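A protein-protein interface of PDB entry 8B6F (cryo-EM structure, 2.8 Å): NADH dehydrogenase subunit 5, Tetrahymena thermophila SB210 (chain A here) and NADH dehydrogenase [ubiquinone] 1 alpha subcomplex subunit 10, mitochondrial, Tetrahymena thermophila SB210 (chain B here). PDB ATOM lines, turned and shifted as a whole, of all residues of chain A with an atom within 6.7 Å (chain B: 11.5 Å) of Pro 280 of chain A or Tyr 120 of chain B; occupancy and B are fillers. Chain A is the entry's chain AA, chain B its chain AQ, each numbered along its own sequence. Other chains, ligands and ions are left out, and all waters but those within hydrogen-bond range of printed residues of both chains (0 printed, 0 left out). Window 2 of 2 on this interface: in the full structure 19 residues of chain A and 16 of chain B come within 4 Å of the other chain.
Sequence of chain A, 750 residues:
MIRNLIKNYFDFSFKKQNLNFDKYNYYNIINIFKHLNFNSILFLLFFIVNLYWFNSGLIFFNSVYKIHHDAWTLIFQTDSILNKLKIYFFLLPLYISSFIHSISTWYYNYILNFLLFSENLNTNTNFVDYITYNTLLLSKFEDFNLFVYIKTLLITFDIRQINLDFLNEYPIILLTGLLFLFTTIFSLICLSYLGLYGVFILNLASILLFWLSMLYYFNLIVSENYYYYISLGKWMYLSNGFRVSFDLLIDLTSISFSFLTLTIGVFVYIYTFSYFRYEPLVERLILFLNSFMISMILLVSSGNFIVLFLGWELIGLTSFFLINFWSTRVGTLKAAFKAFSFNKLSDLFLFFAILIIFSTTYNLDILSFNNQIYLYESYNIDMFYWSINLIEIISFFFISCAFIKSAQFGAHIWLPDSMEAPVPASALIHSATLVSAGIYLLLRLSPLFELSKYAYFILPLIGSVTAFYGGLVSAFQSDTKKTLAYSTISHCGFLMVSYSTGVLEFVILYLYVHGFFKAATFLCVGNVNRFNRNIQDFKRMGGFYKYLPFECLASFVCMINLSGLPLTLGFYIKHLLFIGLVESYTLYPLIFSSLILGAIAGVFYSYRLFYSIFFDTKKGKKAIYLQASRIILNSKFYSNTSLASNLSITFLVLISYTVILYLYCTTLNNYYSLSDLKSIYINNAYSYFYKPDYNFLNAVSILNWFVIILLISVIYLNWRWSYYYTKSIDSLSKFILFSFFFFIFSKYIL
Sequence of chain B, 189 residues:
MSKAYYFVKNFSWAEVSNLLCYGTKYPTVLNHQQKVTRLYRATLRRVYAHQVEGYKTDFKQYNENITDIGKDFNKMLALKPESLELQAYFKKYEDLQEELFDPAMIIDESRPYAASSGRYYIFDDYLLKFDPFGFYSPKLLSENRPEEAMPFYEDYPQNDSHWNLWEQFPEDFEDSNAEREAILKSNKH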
ATOM      1  N   PHE A 276      33.738  -2.803 -12.506  1.00  0.00           N
ATOM      2  CA  PHE A 276      33.597  -2.699 -11.063  1.00  0.00           C
ATOM      3  C   PHE A 276      34.902  -2.998 -10.341  1.00  0.00           C
ATOM      4  O   PHE A 276      34.889  -3.364  -9.162  1.00  0.00           O
ATOM      5  CB  PHE A 276      32.481  -3.626 -10.580  1.00  0.00           C
ATOM      6  CG  PHE A 276      31.340  -2.901  -9.933  1.00  0.00           C
ATOM      7  CD1 PHE A 276      30.636  -1.933 -10.630  1.00  0.00           C
ATOM      8  CD2 PHE A 276      30.970  -3.189  -8.632  1.00  0.00           C
ATOM      9  CE1 PHE A 276      29.587  -1.263 -10.039  1.00  0.00           C
ATOM     10  CE2 PHE A 276      29.921  -2.520  -8.035  1.00  0.00           C
ATOM     11  CZ  PHE A 276      29.228  -1.556  -8.740  1.00  0.00           C
ATOM     12  N   TYR A 278      38.035  -2.812  -8.145  1.00  0.00           N
ATOM     13  CA  TYR A 278      38.333  -2.119  -6.892  1.00  0.00           C
ATOM     14  C   TYR A 278      37.076  -1.604  -6.199  1.00  0.00           C
ATOM     15  O   TYR A 278      37.135  -0.631  -5.446  1.00  0.00           O
ATOM     16  CB  TYR A 278      39.306  -0.958  -7.114  1.00  0.00           C
ATOM     17  CG  TYR A 278      40.541  -1.333  -7.889  1.00  0.00           C
ATOM     18  CD1 TYR A 278      41.076  -2.612  -7.810  1.00  0.00           C
ATOM     19  CD2 TYR A 278      41.174  -0.406  -8.702  1.00  0.00           C
ATOM     20  CE1 TYR A 278      42.205  -2.957  -8.521  1.00  0.00           C
ATOM     21  CE2 TYR A 278      42.302  -0.740  -9.417  1.00  0.00           C
ATOM     22  CZ  TYR A 278      42.813  -2.018  -9.324  1.00  0.00           C
ATOM     23  OH  TYR A 278      43.941  -2.353 -10.033  1.00  0.00           O
ATOM     24  N   GLU A 279      35.947  -2.241  -6.435  1.00  0.00           N
ATOM     25  CA  GLU A 279      34.717  -1.834  -5.780  1.00  0.00           C
ATOM     26  C   GLU A 279      34.438  -2.720  -4.573  1.00  0.00           C
ATOM     27  O   GLU A 279      34.855  -3.882  -4.537  1.00  0.00           O
ATOM     28  CB  GLU A 279      33.537  -1.916  -6.750  1.00  0.00           C
ATOM     29  CG  GLU A 279      33.613  -0.931  -7.903  1.00  0.00           C
ATOM     30  CD  GLU A 279      33.366   0.497  -7.470  1.00  0.00           C
ATOM     31  OE1 GLU A 279      33.114   0.722  -6.270  1.00  0.00           O
ATOM     32  OE2 GLU A 279      33.416   1.396  -8.334  1.00  0.00           O
ATOM     33  N   PRO A 280      33.731  -2.205  -3.564  1.00  0.00           N
ATOM     34  CA  PRO A 280      33.448  -3.039  -2.385  1.00  0.00           C
ATOM     35  C   PRO A 280      32.690  -4.307  -2.720  1.00  0.00           C
ATOM     36  O   PRO A 280      32.939  -5.355  -2.112  1.00  0.00           O
ATOM     37  CB  PRO A 280      32.618  -2.112  -1.484  1.00  0.00           C
ATOM     38  CG  PRO A 280      32.837  -0.746  -2.001  1.00  0.00           C
ATOM     39  CD  PRO A 280      33.120  -0.871  -3.456  1.00  0.00           C
ATOM     40  N   LEU A 281      31.769  -4.239  -3.678  1.00  0.00           N
ATOM     41  CA  LEU A 281      30.840  -5.325  -3.975  1.00  0.00           C
ATOM     42  C   LEU A 281      30.881  -5.612  -5.470  1.00  0.00           C
ATOM     43  O   LEU A 281      30.089  -5.061  -6.239  1.00  0.00           O
ATOM     44  CB  LEU A 281      29.439  -4.947  -3.518  1.00  0.00           C
ATOM     45  CG  LEU A 281      29.323  -4.543  -2.049  1.00  0.00           C
ATOM     46  CD1 LEU A 281      28.024  -3.809  -1.820  1.00  0.00           C
ATOM     47  CD2 LEU A 281      29.417  -5.763  -1.147  1.00  0.00           C
ATOM     48  N   VAL A 282      31.799  -6.480  -5.877  1.00  0.00           N
ATOM     49  CA  VAL A 282      31.860  -6.963  -7.249  1.00  0.00           C
ATOM     50  C   VAL A 282      31.156  -8.304  -7.392  1.00  0.00           C
ATOM     51  O   VAL A 282      30.519  -8.568  -8.412  1.00  0.00           O
ATOM     52  CB  VAL A 282      33.328  -7.052  -7.720  1.00  0.00           C
ATOM     53  CG1 VAL A 282      33.396  -7.464  -9.184  1.00  0.00           C
ATOM     54  CG2 VAL A 282      34.037  -5.730  -7.499  1.00  0.00           C
ATOM     55  N   GLU A 283      31.269  -9.159  -6.377  1.00  0.00           N
ATOM     56  CA  GLU A 283      30.585 -10.445  -6.413  1.00  0.00           C
ATOM     57  C   GLU A 283      29.076 -10.257  -6.468  1.00  0.00           C
ATOM     58  O   GLU A 283      28.378 -10.976  -7.190  1.00  0.00           O
ATOM     59  CB  GLU A 283      30.972 -11.288  -5.197  1.00  0.00           C
ATOM     60  CG  GLU A 283      32.470 -11.368  -4.930  1.00  0.00           C
ATOM     61  CD  GLU A 283      32.960 -10.274  -3.999  1.00  0.00           C
ATOM     62  OE1 GLU A 283      32.243  -9.265  -3.835  1.00  0.00           O
ATOM     63  OE2 GLU A 283      34.061 -10.420  -3.429  1.00  0.00           O
ATOM     64  N   TRP A 326      22.870   0.235  -5.745  1.00  0.00           N
ATOM     65  CA  TRP A 326      23.357   1.208  -4.766  1.00  0.00           C
ATOM     66  C   TRP A 326      22.299   1.368  -3.673  1.00  0.00           C
ATOM     67  O   TRP A 326      21.618   2.388  -3.551  1.00  0.00           O
ATOM     68  CB  TRP A 326      23.680   2.533  -5.444  1.00  0.00           C
ATOM     69  CG  TRP A 326      24.715   2.419  -6.525  1.00  0.00           C
ATOM     70  CD1 TRP A 326      24.521   2.590  -7.864  1.00  0.00           C
ATOM     71  CD2 TRP A 326      26.102   2.101  -6.359  1.00  0.00           C
ATOM     72  NE1 TRP A 326      25.701   2.404  -8.542  1.00  0.00           N
ATOM     73  CE2 TRP A 326      26.687   2.101  -7.640  1.00  0.00           C
ATOM     74  CE3 TRP A 326      26.907   1.816  -5.251  1.00  0.00           C
ATOM     75  CZ2 TRP A 326      28.037   1.830  -7.844  1.00  0.00           C
ATOM     76  CZ3 TRP A 326      28.247   1.548  -5.455  1.00  0.00           C
ATOM     77  CH2 TRP A 326      28.800   1.558  -6.742  1.00  0.00           C
ATOM     78  N   THR A 328      22.491   1.795  -0.524  1.00  0.00           N
ATOM     79  CA  THR A 328      22.690   2.793   0.521  1.00  0.00           C
ATOM     80  C   THR A 328      21.973   4.092   0.187  1.00  0.00           C
ATOM     81  O   THR A 328      21.434   4.759   1.077  1.00  0.00           O
ATOM     82  CB  THR A 328      24.177   3.060   0.730  1.00  0.00           C
ATOM     83  OG1 THR A 328      24.762   3.464  -0.510  1.00  0.00           O
ATOM     84  CG2 THR A 328      24.880   1.814   1.238  1.00  0.00           C
ATOM     85  N   ARG A 329      21.964   4.473  -1.087  1.00  0.00           N
ATOM     86  CA  ARG A 329      21.300   5.698  -1.505  1.00  0.00           C
ATOM     87  C   ARG A 329      19.808   5.466  -1.682  1.00  0.00           C
ATOM     88  O   ARG A 329      19.383   4.463  -2.261  1.00  0.00           O
ATOM     89  CB  ARG A 329      21.896   6.206  -2.818  1.00  0.00           C
ATOM     90  CG  ARG A 329      23.255   6.863  -2.678  1.00  0.00           C
ATOM     91  CD  ARG A 329      23.836   7.220  -4.038  1.00  0.00           C
ATOM     92  NE  ARG A 329      22.839   7.809  -4.924  1.00  0.00           N
ATOM     93  CZ  ARG A 329      22.449   9.076  -4.884  1.00  0.00           C
ATOM     94  NH1 ARG A 329      22.946   9.926  -4.001  1.00  0.00           N
ATOM     95  NH2 ARG A 329      21.537   9.501  -5.753  1.00  0.00           N
ATOM     96  N   ASN A 534      32.992   8.785 -13.272  1.00  0.00           N
ATOM     97  CA  ASN A 534      31.550   8.678 -13.069  1.00  0.00           C
ATOM     98  C   ASN A 534      30.780   9.892 -13.570  1.00  0.00           C
ATOM     99  O   ASN A 534      29.586  10.021 -13.269  1.00  0.00           O
ATOM    100  CB  ASN A 534      31.203   8.442 -11.596  1.00  0.00           C
ATOM    101  CG  ASN A 534      31.800   7.159 -11.056  1.00  0.00           C
ATOM    102  OD1 ASN A 534      32.523   7.167 -10.061  1.00  0.00           O
ATOM    103  ND2 ASN A 534      31.495   6.045 -11.713  1.00  0.00           N
ATOM    104  N   GLU B 109      30.522  15.539  -8.205  1.00  0.00           N
ATOM    105  CA  GLU B 109      30.418  14.427  -7.270  1.00  0.00           C
ATOM    106  C   GLU B 109      30.858  14.796  -5.860  1.00  0.00           C
ATOM    107  O   GLU B 109      30.624  14.013  -4.934  1.00  0.00           O
ATOM    108  CB  GLU B 109      31.256  13.247  -7.766  1.00  0.00           C
ATOM    109  CG  GLU B 109      31.039  12.874  -9.230  1.00  0.00           C
ATOM    110  CD  GLU B 109      29.646  12.341  -9.518  1.00  0.00           C
ATOM    111  OE1 GLU B 109      28.666  12.871  -8.956  1.00  0.00           O
ATOM    112  OE2 GLU B 109      29.530  11.386 -10.312  1.00  0.00           O
ATOM    113  N   ALA B 114      24.430  14.502  -4.617  1.00  0.00           N
ATOM    114  CA  ALA B 114      24.808  14.252  -5.996  1.00  0.00           C
ATOM    115  C   ALA B 114      24.784  12.757  -6.287  1.00  0.00           C
ATOM    116  O   ALA B 114      24.739  11.921  -5.382  1.00  0.00           O
ATOM    117  CB  ALA B 114      26.195  14.820  -6.286  1.00  0.00           C
ATOM    118  N   ALA B 115      24.799  12.424  -7.573  1.00  0.00           N
ATOM    119  CA  ALA B 115      24.929  11.029  -7.963  1.00  0.00           C
ATOM    120  C   ALA B 115      26.250  10.482  -7.441  1.00  0.00           C
ATOM    121  O   ALA B 115      27.307  11.088  -7.637  1.00  0.00           O
ATOM    122  CB  ALA B 115      24.854  10.894  -9.483  1.00  0.00           C
ATOM    123  N   SER B 116      26.191   9.333  -6.774  1.00  0.00           N
ATOM    124  CA  SER B 116      27.332   8.694  -6.127  1.00  0.00           C
ATOM    125  C   SER B 116      27.671   9.355  -4.798  1.00  0.00           C
ATOM    126  O   SER B 116      28.734   9.070  -4.229  1.00  0.00           O
ATOM    127  CB  SER B 116      28.581   8.695  -7.015  1.00  0.00           C
ATOM    128  OG  SER B 116      29.075  10.010  -7.204  1.00  0.00           O
ATOM    129  N   SER B 117      26.805  10.229  -4.282  1.00  0.00           N
ATOM    130  CA  SER B 117      27.118  10.949  -3.053  1.00  0.00           C
ATOM    131  C   SER B 117      27.233  10.006  -1.860  1.00  0.00           C
ATOM    132  O   SER B 117      28.149  10.143  -1.041  1.00  0.00           O
ATOM    133  CB  SER B 117      26.053  12.012  -2.789  1.00  0.00           C
ATOM    134  OG  SER B 117      26.282  12.664  -1.553  1.00  0.00           O
ATOM    135  N   GLY B 118      26.319   9.048  -1.745  1.00  0.00           N
ATOM    136  CA  GLY B 118      26.257   8.199  -0.571  1.00  0.00           C
ATOM    137  C   GLY B 118      26.279   6.720  -0.891  1.00  0.00           C
ATOM    138  O   GLY B 118      25.591   5.927  -0.242  1.00  0.00           O
ATOM    139  N   ARG B 119      27.067   6.334  -1.893  1.00  0.00           N
ATOM    140  CA  ARG B 119      27.091   4.942  -2.323  1.00  0.00           C
ATOM    141  C   ARG B 119      27.634   4.000  -1.259  1.00  0.00           C
ATOM    142  O   ARG B 119      27.397   2.792  -1.351  1.00  0.00           O
ATOM    143  CB  ARG B 119      27.919   4.800  -3.597  1.00  0.00           C
ATOM    144  CG  ARG B 119      27.187   5.243  -4.843  1.00  0.00           C
ATOM    145  CD  ARG B 119      28.119   5.277  -6.041  1.00  0.00           C
ATOM    146  NE  ARG B 119      27.424   5.649  -7.265  1.00  0.00           N
ATOM    147  CZ  ARG B 119      27.995   5.707  -8.461  1.00  0.00           C
ATOM    148  NH1 ARG B 119      29.274   5.420  -8.630  1.00  0.00           N
ATOM    149  NH2 ARG B 119      27.262   6.060  -9.513  1.00  0.00           N
ATOM    150  N   TYR B 120      28.355   4.506  -0.263  1.00  0.00           N
ATOM    151  CA  TYR B 120      29.024   3.657   0.711  1.00  0.00           C
ATOM    152  C   TYR B 120      28.687   4.108   2.124  1.00  0.00           C
ATOM    153  O   TYR B 120      28.578   5.307   2.394  1.00  0.00           O
ATOM    154  CB  TYR B 120      30.537   3.673   0.492  1.00  0.00           C
ATOM    155  CG  TYR B 120      30.909   3.548  -0.965  1.00  0.00           C
ATOM    156  CD1 TYR B 120      30.942   2.312  -1.590  1.00  0.00           C
ATOM    157  CD2 TYR B 120      31.212   4.672  -1.720  1.00  0.00           C
ATOM    158  CE1 TYR B 120      31.274   2.194  -2.924  1.00  0.00           C
ATOM    159  CE2 TYR B 120      31.545   4.566  -3.055  1.00  0.00           C
ATOM    160  CZ  TYR B 120      31.572   3.324  -3.650  1.00  0.00           C
ATOM    161  OH  TYR B 120      31.906   3.213  -4.979  1.00  0.00           O
ATOM    162  N   TYR B 121      28.519   3.137   3.018  1.00  0.00           N
ATOM    163  CA  TYR B 121      28.251   3.392   4.427  1.00  0.00           C
ATOM    164  C   TYR B 121      29.532   3.149   5.214  1.00  0.00           C
ATOM    165  O   TYR B 121      30.042   2.025   5.245  1.00  0.00           O
ATOM    166  CB  TYR B 121      27.124   2.494   4.936  1.00  0.00           C
ATOM    167  CG  TYR B 121      26.910   2.559   6.431  1.00  0.00           C
ATOM    168  CD1 TYR B 121      26.397   3.699   7.034  1.00  0.00           C
ATOM    169  CD2 TYR B 121      27.205   1.469   7.235  1.00  0.00           C
ATOM    170  CE1 TYR B 121      26.196   3.755   8.399  1.00  0.00           C
ATOM    171  CE2 TYR B 121      27.006   1.515   8.599  1.00  0.00           C
ATOM    172  CZ  TYR B 121      26.501   2.659   9.174  1.00  0.00           C
ATOM    173  OH  TYR B 121      26.303   2.705  10.533  1.00  0.00           O
ATOM    174  N   ILE B 122      30.042   4.199   5.848  1.00  0.00           N
ATOM    175  CA  ILE B 122      31.304   4.134   6.574  1.00  0.00           C
ATOM    176  C   ILE B 122      31.025   3.702   8.006  1.00  0.00           C
ATOM    177  O   ILE B 122      30.195   4.304   8.696  1.00  0.00           O
ATOM    178  CB  ILE B 122      32.024   5.492   6.536  1.00  0.00           C
ATOM    179  CG1 ILE B 122      32.082   6.032   5.105  1.00  0.00           C
ATOM    180  CG2 ILE B 122      33.425   5.368   7.110  1.00  0.00           C
ATOM    181  CD1 ILE B 122      32.716   5.090   4.106  1.00  0.00           C
ATOM    182  N   PHE B 123      31.720   2.660   8.454  1.00  0.00           N
ATOM    183  CA  PHE B 123      31.487   2.112   9.782  1.00  0.00           C
ATOM    184  C   PHE B 123      32.281   2.883  10.828  1.00  0.00           C
ATOM    185  O   PHE B 123      33.465   3.178  10.641  1.00  0.00           O
ATOM    186  CB  PHE B 123      31.865   0.633   9.817  1.00  0.00           C
ATOM    187  CG  PHE B 123      31.032  -0.221   8.909  1.00  0.00           C
ATOM    188  CD1 PHE B 123      29.822  -0.736   9.339  1.00  0.00           C
ATOM    189  CD2 PHE B 123      31.458  -0.508   7.624  1.00  0.00           C
ATOM    190  CE1 PHE B 123      29.052  -1.523   8.507  1.00  0.00           C
ATOM    191  CE2 PHE B 123      30.692  -1.293   6.786  1.00  0.00           C
ATOM    192  CZ  PHE B 123      29.487  -1.802   7.229  1.00  0.00           C
ATOM    193  N   ASP B 124      31.618   3.202  11.936  1.00  0.00           N
ATOM    194  CA  ASP B 124      32.210   4.000  12.998  1.00  0.00           C
ATOM    195  C   ASP B 124      33.046   3.126  13.928  1.00  0.00           C
ATOM    196  O   ASP B 124      32.919   1.900  13.955  1.00  0.00           O
ATOM    197  CB  ASP B 124      31.119   4.713  13.795  1.00  0.00           C
ATOM    198  CG  ASP B 124      31.676   5.744  14.754  1.00  0.00           C
ATOM    199  OD1 ASP B 124      32.098   6.823  14.289  1.00  0.00           O
ATOM    200  OD2 ASP B 124      31.693   5.478  15.973  1.00  0.00           O
ATOM    201  N   LEU B 127      31.153   0.508  15.940  1.00  0.00           N
ATOM    202  CA  LEU B 127      30.923  -0.775  15.283  1.00  0.00           C
ATOM    203  C   LEU B 127      32.215  -1.571  15.155  1.00  0.00           C
ATOM    204  O   LEU B 127      32.212  -2.796  15.316  1.00  0.00           O
ATOM    205  CB  LEU B 127      30.292  -0.553  13.909  1.00  0.00           C
ATOM    206  CG  LEU B 127      28.870   0.010  13.928  1.00  0.00           C
ATOM    207  CD1 LEU B 127      28.414   0.350  12.524  1.00  0.00           C
ATOM    208  CD2 LEU B 127      27.907  -0.972  14.573  1.00  0.00           C
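Of chain B, only Tyr 120 comes within 4 Å of Pro 280 of chain A.
Of the printed residues of chain A, Tyr 120 of chain B touches Glu 279, Pro 280, Trp 326 and Thr 328.
No residue of chain B comes within 4 Å of Val 282 of chain A.
Printed residues of chain B within 4 Å of Thr 328 of chain A: Gly 118 (2.6 Å), Arg 119 (2.8 Å) and Tyr 120 (3.7 Å).
Printed residues of chain A within 4 Å of Ser 117 of chain B: Arg 329 (3.9 Å).
Printed residues of chain A within 4 Å of Ala 114 of chain B: Arg 329.
The nearest residue of chain A that does not touch Tyr 120 of chain B is Arg 329 of chain A (6.1 Å).
The nearest printed residue of chain B that does not touch Asn 534 of chain A is Ser 116 of chain B (5.1 Å).
Tyr 120 of chain B touches Pro 280 of chain A (CE1 to CG, 3.5 Å).
Trp 326 of chain A touches Arg 119 of chain B.
Tyr 120 of chain B touches Trp 326 of chain A (OH to CH2, 3.9 Å).
OG1 of Thr 328 of chain A touches N of Tyr 120 of chain B, 3.7 Å away.
N of Ser 117 of chain B touches NH1 of Arg 329 of chain A (3.9 Å).
Arg 329 of chain A touches Gly 118 of chain B (CG to O, 3.5 Å).
Arg 119 of chain B touches Arg 329 of chain A (N to CG, 3.9 Å).
ND2 of Asn 534 of chain A touches NH1 of Arg 119 of chain B, 3.9 Å away.
O of Ala 115 of chain B sits close to OE1 of Glu 109 of chain B (2.6 Å).
The side-chain hydroxyl of Ser 116 of chain B sits close to the side-chain carboxylate of Glu 109 of chain B.
Of the 13 printed residues of chain B, 6 touch a printed residue of chain A.
Hydrophobic or aromatic side chains of chain B that line the printed part of chain A: Tyr 120.
Printed residues of chain A that touch a printed residue of chain B: Glu 279, Pro 280, Trp 326, Thr 328, Arg 329 and Asn 534.
Among the printed residues, 13 pairs touch across the chains.
Among the printed residues, no Asp or Glu carboxylate lies within 4 Å of a Lys or Arg side-chain nitrogen of the other chain.
The side-chain hydroxyl of Tyr 120 of chain B sits at hydrogen-bond distance from the side-chain carboxylate of Glu 279 of chain A (3.1 Å).
OG1 of Thr 328 of chain A is in hydrogen-bond range of O of Gly 118 of chain B (2.6 Å).
OG1 of Thr 328 of chain A sits at hydrogen-bond distance from O of Arg 119 of chain B, at 2.8 Å.
The guanidinium group (NH1) of Arg 329 of chain A sits at hydrogen-bond distance from the backbone carbonyl oxygen (O) of Ala 114 of chain B (3.0 Å).
OE2 of Glu 109 of chain B sits close to O of Asn 534 of chain A (3.3 Å).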
